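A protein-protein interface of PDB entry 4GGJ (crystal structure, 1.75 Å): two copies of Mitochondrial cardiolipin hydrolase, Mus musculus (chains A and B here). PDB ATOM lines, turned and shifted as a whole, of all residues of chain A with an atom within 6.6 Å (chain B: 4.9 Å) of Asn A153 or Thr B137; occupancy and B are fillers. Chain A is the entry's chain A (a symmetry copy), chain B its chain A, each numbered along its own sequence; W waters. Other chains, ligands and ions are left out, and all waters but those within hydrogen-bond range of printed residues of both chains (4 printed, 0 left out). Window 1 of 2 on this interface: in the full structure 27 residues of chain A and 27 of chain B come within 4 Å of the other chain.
The backbone NH (N) of His B125 is in hydrogen-bond range of the backbone carbonyl oxygen (O) of Arg A151.
A ring nitrogen (ND1) of His B125 sits at hydrogen-bond distance from the side-chain amide oxygen of Asn A153.
The backbone carbonyl oxygen (O) of Lys B126 lies within hydrogen-bond range of the backbone NH (N) of Gly B138 (3.1 Å).
The backbone NH (N) of Met B157 sits at hydrogen-bond distance from the backbone carbonyl oxygen (O) of Leu B135 (2.8 Å).
N of Ser B139 is in hydrogen-bond range of O of Asn B153.
N of Leu A155 lies within hydrogen-bond range of O of Thr A137 (2.7 Å).
The side-chain carboxylate (OE1) of Glu A152 sits at hydrogen-bond distance from the side-chain hydroxyl (OG) of Ser A139, 2.7 Å away.
The backbone NH (N) of Leu A140 lies close to the side-chain carboxylate (OE1) of Glu A152 (3.4 Å).
CG2 of Val A11 touches CE1 of Phe B166, at 3.6 Å.
His B125 touches Phe A13 (CE1 to CD1, 3.97 Å).
CZ of Phe A13 touches CD1 of Phe B166, 3.97 Å away.
Thr A137 touches Asn B153 (OG1 to ND2, 3.7 Å).
Lys B126 touches Ser A139.
Thr B137 touches Asn A153 (OG1 to ND2, 3.7 Å).
Phe B166 touches Asn A153.
Leu B155 touches Leu A155.
CD1 of Leu A155 touches CE of Met B157 (3.7 Å).
Phe B166 touches Leu A155 (CE1 to CD2, 3.8 Å).
Of the printed residues of chain B, Thr A137 touches Asn B153.
Asn A153 touches three residues of chain B.
Of the printed residues of chain B, Leu A155 touches Leu B155, Met B157 and Phe B166.
Ile B136 touches none of the printed residues of chain A.
Of the printed residues of chain A, Thr B137 touches Asn A153 (3.7 Å).
Gly B138 touches none of the printed residues of chain A.
Printed residues of chain A within 4 Å of Leu B155: Leu A155.
Of the printed residues of chain A, Met B157 touches Leu A155.
The nearest residue of chain A that does not touch Thr B137 is Leu A155 (4.1 Å).
The nearest printed residue of chain B that does not touch Arg A151 is Lys B126 (6.7 Å).
Of the 13 printed residues of chain A, 8 touch a printed residue of chain B.
Hydrophobic or aromatic side chains of chain A that line the printed part of chain B: Val A11, Phe A13 and Leu A155.
Hydrophobic or aromatic side chains of chain B that line the printed part of chain A: His B125, Leu B155, Met B157 and Phe B166.
Among the printed residues, 13 pairs touch across the chains.
Among the printed residues, no Asp or Glu carboxylate lies within 4 Å of a Lys or Arg side-chain nitrogen of the other chain.
Thr A137 touches Asn B153, and with the chains exchanged Asn A153 touches Thr B137.
Leu A155 touches its own counterpart, Leu B155.
6 positions are printed for both chains.
Of the 13 pairs that touch across the chains among the printed residues, 3 have their exchanged pair printed and touching as well.
Water W2 lies within hydrogen-bond range of the side-chain amide nitrogen of Asn B153 and the side-chain hydroxyl of Thr A137.
Water W4 bridges ND2 of Asn A153 (2.6 Å) and OG1 of Thr B137 (2.7 Å).
Water W1 lies within hydrogen-bond range of OG1 of Thr B137 (2.9 Å), O of Gly B138 (2.9 Å), N of Lys B126 (3.0 Å) and OD1 of Asn A153 (3.0 Å).
Water W3 lies within hydrogen-bond range of the side-chain hydroxyl (OG1) of Thr A137, the backbone carbonyl oxygen (O) of Gly A138 and the side-chain amide oxygen (OD1) of Asn B153.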
ATOM      1  N   VAL A  11      -2.924   6.730  12.908  1.00  0.00           N
ATOM      2  CA  VAL A  11      -1.479   6.561  12.804  1.00  0.00           C
ATOM      3  C   VAL A  11      -1.181   5.104  12.457  1.00  0.00           C
ATOM      4  O   VAL A  11      -1.759   4.143  13.046  1.00  0.00           O
ATOM      5  CB  VAL A  11      -0.717   6.992  14.089  1.00  0.00           C
ATOM      6  CG1 VAL A  11      -1.250   6.300  15.309  1.00  0.00           C
ATOM      7  CG2 VAL A  11       0.801   6.719  13.924  1.00  0.00           C
ATOM      8  N   LEU A  12      -0.303   4.955  11.478  1.00  0.00           N
ATOM      9  CA  LEU A  12       0.179   3.675  11.032  1.00  0.00           C
ATOM     10  C   LEU A  12       1.613   3.548  11.512  1.00  0.00           C
ATOM     11  O   LEU A  12       2.422   4.469  11.284  1.00  0.00           O
ATOM     12  CB  LEU A  12       0.179   3.606   9.507  1.00  0.00           C
ATOM     13  CG  LEU A  12      -1.097   3.970   8.733  1.00  0.00           C
ATOM     14  CD1 LEU A  12      -0.877   3.793   7.226  1.00  0.00           C
ATOM     15  CD2 LEU A  12      -2.251   3.212   9.231  1.00  0.00           C
ATOM     16  N   PHE A  13       1.931   2.421  12.144  1.00  0.00           N
ATOM     17  CA  PHE A  13       3.304   2.139  12.520  1.00  0.00           C
ATOM     18  C   PHE A  13       3.872   1.043  11.644  1.00  0.00           C
ATOM     19  O   PHE A  13       3.187   0.071  11.276  1.00  0.00           O
ATOM     20  CB  PHE A  13       3.401   1.760  13.992  1.00  0.00           C
ATOM     21  CG  PHE A  13       3.078   2.898  14.944  1.00  0.00           C
ATOM     22  CD1 PHE A  13       3.959   3.958  15.090  1.00  0.00           C
ATOM     23  CD2 PHE A  13       1.928   2.883  15.710  1.00  0.00           C
ATOM     24  CE1 PHE A  13       3.684   4.993  15.973  1.00  0.00           C
ATOM     25  CE2 PHE A  13       1.639   3.917  16.597  1.00  0.00           C
ATOM     26  CZ  PHE A  13       2.523   4.976  16.729  1.00  0.00           C
ATOM     27  N   PHE A  14       5.138   1.206  11.324  1.00  0.00           N
ATOM     28  CA  PHE A  14       5.868   0.292  10.482  1.00  0.00           C
ATOM     29  C   PHE A  14       6.980  -0.285  11.344  1.00  0.00           C
ATOM     30  O   PHE A  14       7.349   0.312  12.345  1.00  0.00           O
ATOM     31  CB  PHE A  14       6.419   1.060   9.273  1.00  0.00           C
ATOM     32  CG  PHE A  14       5.351   1.532   8.330  1.00  0.00           C
ATOM     33  CD1 PHE A  14       4.596   2.669   8.629  1.00  0.00           C
ATOM     34  CD2 PHE A  14       5.071   0.836   7.173  1.00  0.00           C
ATOM     35  CE1 PHE A  14       3.597   3.104   7.785  1.00  0.00           C
ATOM     36  CE2 PHE A  14       4.057   1.284   6.307  1.00  0.00           C
ATOM     37  CZ  PHE A  14       3.334   2.430   6.624  1.00  0.00           C
ATOM     38  N   THR A 137       1.231  12.112   6.458  1.00  0.00           N
ATOM     39  CA  THR A 137       2.582  12.618   6.695  1.00  0.00           C
ATOM     40  C   THR A 137       3.282  11.754   7.714  1.00  0.00           C
ATOM     41  O   THR A 137       2.697  11.366   8.720  1.00  0.00           O
ATOM     42  CB  THR A 137       2.598  14.107   7.095  1.00  0.00           C
ATOM     43  OG1 THR A 137       3.956  14.581   7.201  1.00  0.00           O
ATOM     44  CG2 THR A 137       1.846  14.370   8.406  1.00  0.00           C
ATOM     45  N   GLY A 138       4.538  11.450   7.450  1.00  0.00           N
ATOM     46  CA  GLY A 138       5.307  10.715   8.441  1.00  0.00           C
ATOM     47  C   GLY A 138       6.802  10.764   8.342  1.00  0.00           C
ATOM     48  O   GLY A 138       7.375  11.603   7.653  1.00  0.00           O
ATOM     49  N   SER A 139       7.423   9.817   9.037  1.00  0.00           N
ATOM     50  CA  SER A 139       8.867   9.621   8.969  1.00  0.00           C
ATOM     51  C   SER A 139       9.244   8.755   7.765  1.00  0.00           C
ATOM     52  O   SER A 139      10.414   8.714   7.373  1.00  0.00           O
ATOM     53  CB  SER A 139       9.360   8.931  10.247  1.00  0.00           C
ATOM     54  OG  SER A 139       8.799   7.627  10.337  1.00  0.00           O
ATOM     55  N   LEU A 140       8.259   8.072   7.180  1.00  0.00           N
ATOM     56  CA  LEU A 140       8.499   6.983   6.207  1.00  0.00           C
ATOM     57  C   LEU A 140       8.841   7.492   4.817  1.00  0.00           C
ATOM     58  O   LEU A 140       8.061   8.227   4.217  1.00  0.00           O
ATOM     59  CB  LEU A 140       7.244   6.102   6.115  1.00  0.00           C
ATOM     60  CG  LEU A 140       7.204   4.953   5.088  1.00  0.00           C
ATOM     61  CD1 LEU A 140       8.078   3.750   5.543  1.00  0.00           C
ATOM     62  CD2 LEU A 140       5.790   4.512   4.826  1.00  0.00           C
ATOM     63  N   ARG A 151      11.276   0.997  11.697  1.00  0.00           N
ATOM     64  CA  ARG A 151      10.338   1.585  12.609  1.00  0.00           C
ATOM     65  C   ARG A 151      10.056   2.997  12.095  1.00  0.00           C
ATOM     66  O   ARG A 151      10.982   3.803  11.939  1.00  0.00           O
ATOM     67  CB  ARG A 151      10.948   1.633  14.012  1.00  0.00           C
ATOM     68  CG  ARG A 151      11.351   0.272  14.575  1.00  0.00           C
ATOM     69  CD  ARG A 151      10.128  -0.568  14.971  1.00  0.00           C
ATOM     70  NE  ARG A 151      10.318  -1.228  16.266  1.00  0.00           N
ATOM     71  CZ  ARG A 151       9.391  -1.923  16.925  1.00  0.00           C
ATOM     72  NH1 ARG A 151       8.163  -2.073  16.426  1.00  0.00           N
ATOM     73  NH2 ARG A 151       9.700  -2.472  18.098  1.00  0.00           N
ATOM     74  N   GLU A 152       8.798   3.248  11.759  1.00  0.00           N
ATOM     75  CA  GLU A 152       8.348   4.498  11.147  1.00  0.00           C
ATOM     76  C   GLU A 152       6.926   4.770  11.577  1.00  0.00           C
ATOM     77  O   GLU A 152       6.213   3.844  11.999  1.00  0.00           O
ATOM     78  CB  GLU A 152       8.289   4.392   9.619  1.00  0.00           C
ATOM     79  CG  GLU A 152       9.497   3.807   8.902  1.00  0.00           C
ATOM     80  CD  GLU A 152      10.485   4.839   8.458  1.00  0.00           C
ATOM     81  OE1 GLU A 152      10.352   6.030   8.841  1.00  0.00           O
ATOM     82  OE2 GLU A 152      11.426   4.453   7.732  1.00  0.00           O
ATOM     83  N   ASN A 153       6.493   6.016  11.387  1.00  0.00           N
ATOM     84  CA  ASN A 153       5.116   6.394  11.607  1.00  0.00           C
ATOM     85  C   ASN A 153       4.608   7.160  10.380  1.00  0.00           C
ATOM     86  O   ASN A 153       5.376   7.867   9.698  1.00  0.00           O
ATOM     87  CB  ASN A 153       4.962   7.235  12.882  1.00  0.00           C
ATOM     88  CG  ASN A 153       5.679   8.564  12.802  1.00  0.00           C
ATOM     89  OD1 ASN A 153       6.864   8.667  13.173  1.00  0.00           O
ATOM     90  ND2 ASN A 153       4.972   9.592  12.366  1.00  0.00           N
ATOM     91  N   VAL A 154       3.335   6.982  10.086  1.00  0.00           N
ATOM     92  CA  VAL A 154       2.616   7.788   9.117  1.00  0.00           C
ATOM     93  C   VAL A 154       1.289   8.204   9.757  1.00  0.00           C
ATOM     94  O   VAL A 154       0.522   7.352  10.232  1.00  0.00           O
ATOM     95  CB  VAL A 154       2.367   7.024   7.804  1.00  0.00           C
ATOM     96  CG1 VAL A 154       1.469   7.847   6.868  1.00  0.00           C
ATOM     97  CG2 VAL A 154       3.688   6.663   7.104  1.00  0.00           C
ATOM     98  N   LEU A 155       1.052   9.516   9.820  1.00  0.00           N
ATOM     99  CA  LEU A 155      -0.220  10.077  10.290  1.00  0.00           C
ATOM    100  C   LEU A 155      -1.143  10.286   9.105  1.00  0.00           C
ATOM    101  O   LEU A 155      -0.681  10.672   8.035  1.00  0.00           O
ATOM    102  CB  LEU A 155      -0.022  11.426  10.984  1.00  0.00           C
ATOM    103  CG  LEU A 155       0.995  11.503  12.113  1.00  0.00           C
ATOM    104  CD1 LEU A 155       1.085  12.868  12.735  1.00  0.00           C
ATOM    105  CD2 LEU A 155       0.696  10.473  13.175  1.00  0.00           C
ATOM    106  N   HIS B 125      12.012   6.687  13.306  1.00  0.00           N
ATOM    107  CA  HIS B 125      11.176   7.728  13.947  1.00  0.00           C
ATOM    108  C   HIS B 125      11.943   9.034  14.239  1.00  0.00           C
ATOM    109  O   HIS B 125      13.160   9.030  14.501  1.00  0.00           O
ATOM    110  CB  HIS B 125      10.639   7.231  15.288  1.00  0.00           C
ATOM    111  CG  HIS B 125       9.614   6.137  15.187  1.00  0.00           C
ATOM    112  ND1 HIS B 125       8.413   6.291  14.520  1.00  0.00           N
ATOM    113  CD2 HIS B 125       9.597   4.890  15.707  1.00  0.00           C
ATOM    114  CE1 HIS B 125       7.708   5.177  14.626  1.00  0.00           C
ATOM    115  NE2 HIS B 125       8.393   4.314  15.354  1.00  0.00           N
ATOM    116  N   LYS B 126      11.208  10.142  14.223  1.00  0.00           N
ATOM    117  CA  LYS B 126      11.707  11.422  14.686  1.00  0.00           C
ATOM    118  C   LYS B 126      10.671  12.113  15.569  1.00  0.00           C
ATOM    119  O   LYS B 126      10.063  13.158  15.182  1.00  0.00           O
ATOM    120  CB  LYS B 126      12.118  12.337  13.522  1.00  0.00           C
ATOM    121  CG  LYS B 126      12.984  11.720  12.471  1.00  0.00           C
ATOM    122  CD  LYS B 126      12.166  11.226  11.281  1.00  0.00           C
ATOM    123  CE  LYS B 126      13.007  10.992  10.027  1.00  0.00           C
ATOM    124  NZ  LYS B 126      14.175  10.134  10.223  1.00  0.00           N
ATOM    125  N   PHE B 127      10.472  11.547  16.762  1.00  0.00           N
ATOM    126  CA  PHE B 127       9.474  12.106  17.669  1.00  0.00           C
ATOM    127  C   PHE B 127       9.938  12.275  19.099  1.00  0.00           C
ATOM    128  O   PHE B 127      10.937  11.676  19.540  1.00  0.00           O
ATOM    129  CB  PHE B 127       8.115  11.359  17.590  1.00  0.00           C
ATOM    130  CG  PHE B 127       8.092   9.955  18.202  1.00  0.00           C
ATOM    131  CD1 PHE B 127       7.947   9.777  19.575  1.00  0.00           C
ATOM    132  CD2 PHE B 127       8.149   8.826  17.395  1.00  0.00           C
ATOM    133  CE1 PHE B 127       7.883   8.518  20.130  1.00  0.00           C
ATOM    134  CE2 PHE B 127       8.100   7.529  17.959  1.00  0.00           C
ATOM    135  CZ  PHE B 127       7.975   7.386  19.331  1.00  0.00           C
ATOM    136  N   LEU B 135       2.841  15.631  21.785  1.00  0.00           N
ATOM    137  CA  LEU B 135       3.600  14.855  20.815  1.00  0.00           C
ATOM    138  C   LEU B 135       4.228  15.828  19.837  1.00  0.00           C
ATOM    139  O   LEU B 135       3.554  16.691  19.265  1.00  0.00           O
ATOM    140  CB  LEU B 135       2.706  13.893  20.031  1.00  0.00           C
ATOM    141  CG  LEU B 135       3.373  13.148  18.871  1.00  0.00           C
ATOM    142  CD1 LEU B 135       4.451  12.261  19.428  1.00  0.00           C
ATOM    143  CD2 LEU B 135       2.341  12.321  18.080  1.00  0.00           C
ATOM    144  N   ILE B 136       5.524  15.668  19.662  1.00  0.00           N
ATOM    145  CA  ILE B 136       6.308  16.422  18.692  1.00  0.00           C
ATOM    146  C   ILE B 136       6.829  15.409  17.682  1.00  0.00           C
ATOM    147  O   ILE B 136       7.528  14.472  18.047  1.00  0.00           O
ATOM    148  CB  ILE B 136       7.511  17.113  19.365  1.00  0.00           C
ATOM    149  CG1 ILE B 136       7.045  18.097  20.421  1.00  0.00           C
ATOM    150  CG2 ILE B 136       8.393  17.810  18.259  1.00  0.00           C
ATOM    151  CD1 ILE B 136       8.137  18.575  21.315  1.00  0.00           C
ATOM    152  N   THR B 137       6.438  15.527  16.419  1.00  0.00           N
ATOM    153  CA  THR B 137       6.817  14.491  15.460  1.00  0.00           C
ATOM    154  C   THR B 137       6.967  15.095  14.086  1.00  0.00           C
ATOM    155  O   THR B 137       6.154  15.911  13.664  1.00  0.00           O
ATOM    156  CB  THR B 137       5.843  13.295  15.460  1.00  0.00           C
ATOM    157  OG1 THR B 137       6.328  12.256  14.584  1.00  0.00           O
ATOM    158  CG2 THR B 137       4.419  13.698  15.058  1.00  0.00           C
ATOM    159  N   GLY B 138       8.012  14.694  13.388  1.00  0.00           N
ATOM    160  CA  GLY B 138       8.158  15.150  12.016  1.00  0.00           C
ATOM    161  C   GLY B 138       9.061  14.366  11.112  1.00  0.00           C
ATOM    162  O   GLY B 138       9.441  13.236  11.403  1.00  0.00           O
ATOM    163  N   SER B 139       9.420  15.014  10.008  1.00  0.00           N
ATOM    164  CA  SER B 139      10.392  14.470   9.067  1.00  0.00           C
ATOM    165  C   SER B 139      11.821  14.783   9.516  1.00  0.00           C
ATOM    166  O   SER B 139      12.774  14.174   9.022  1.00  0.00           O
ATOM    167  CB  SER B 139      10.168  15.078   7.676  1.00  0.00           C
ATOM    168  OG  SER B 139      10.414  16.478   7.718  1.00  0.00           O
ATOM    169  N   ASN B 153       9.170  19.175   8.151  1.00  0.00           N
ATOM    170  CA  ASN B 153       8.048  19.562   8.975  1.00  0.00           C
ATOM    171  C   ASN B 153       8.193  18.907  10.353  1.00  0.00           C
ATOM    172  O   ASN B 153       8.744  17.796  10.485  1.00  0.00           O
ATOM    173  CB  ASN B 153       6.713  19.177   8.322  1.00  0.00           C
ATOM    174  CG  ASN B 153       6.538  17.683   8.176  1.00  0.00           C
ATOM    175  OD1 ASN B 153       6.927  17.097   7.147  1.00  0.00           O
ATOM    176  ND2 ASN B 153       5.921  17.060   9.164  1.00  0.00           N
ATOM    177  N   VAL B 154       7.738  19.614  11.369  1.00  0.00           N
ATOM    178  CA  VAL B 154       7.572  19.079  12.708  1.00  0.00           C
ATOM    179  C   VAL B 154       6.184  19.495  13.202  1.00  0.00           C
ATOM    180  O   VAL B 154       5.840  20.687  13.191  1.00  0.00           O
ATOM    181  CB  VAL B 154       8.663  19.586  13.670  1.00  0.00           C
ATOM    182  CG1 VAL B 154       8.364  19.129  15.106  1.00  0.00           C
ATOM    183  CG2 VAL B 154      10.060  19.114  13.234  1.00  0.00           C
ATOM    184  N   LEU B 155       5.373  18.504  13.577  1.00  0.00           N
ATOM    185  CA  LEU B 155       4.058  18.734  14.188  1.00  0.00           C
ATOM    186  C   LEU B 155       4.205  18.762  15.696  1.00  0.00           C
ATOM    187  O   LEU B 155       4.991  17.995  16.246  1.00  0.00           O
ATOM    188  CB  LEU B 155       3.064  17.628  13.826  1.00  0.00           C
ATOM    189  CG  LEU B 155       2.870  17.300  12.353  1.00  0.00           C
ATOM    190  CD1 LEU B 155       1.853  16.219  12.118  1.00  0.00           C
ATOM    191  CD2 LEU B 155       2.495  18.536  11.573  1.00  0.00           C
ATOM    192  N   MET B 157       1.515  18.559  18.810  1.00  0.00           N
ATOM    193  CA  MET B 157       0.117  18.232  18.997  1.00  0.00           C
ATOM    194  C   MET B 157      -0.182  17.812  20.418  1.00  0.00           C
ATOM    195  O   MET B 157       0.455  16.915  20.947  1.00  0.00           O
ATOM    196  CB  MET B 157      -0.273  17.082  18.060  1.00  0.00           C
ATOM    197  CG  MET B 157      -0.284  17.471  16.633  1.00  0.00           C
ATOM    198  SD  MET B 157      -0.728  16.052  15.616  1.00  0.00           S
ATOM    199  CE  MET B 157       0.733  15.027  15.753  1.00  0.00           C
ATOM    200  N   PHE B 166       1.718   6.730  20.417  1.00  0.00           N
ATOM    201  CA  PHE B 166       3.172   6.976  20.314  1.00  0.00           C
ATOM    202  C   PHE B 166       3.915   6.554  21.598  1.00  0.00           C
ATOM    203  O   PHE B 166       5.024   5.990  21.517  1.00  0.00           O
ATOM    204  CB  PHE B 166       3.494   8.428  19.915  1.00  0.00           C
ATOM    205  CG  PHE B 166       3.429   8.691  18.416  1.00  0.00           C
ATOM    206  CD1 PHE B 166       2.220   8.794  17.763  1.00  0.00           C
ATOM    207  CD2 PHE B 166       4.592   8.828  17.668  1.00  0.00           C
ATOM    208  CE1 PHE B 166       2.161   9.046  16.353  1.00  0.00           C
ATOM    209  CE2 PHE B 166       4.540   9.077  16.280  1.00  0.00           C
ATOM    210  CZ  PHE B 166       3.324   9.187  15.636  1.00  0.00           C
HETATM  211  O   HOH W   1       8.599  11.121  13.206  1.00  0.00           O
HETATM  212  O   HOH W   2       5.130  14.593   9.670  1.00  0.00           O
HETATM  213  O   HOH W   3       6.722  14.176   6.475  1.00  0.00           O
HETATM  214  O   HOH W   4       5.374  12.178  12.024  1.00  0.00           O
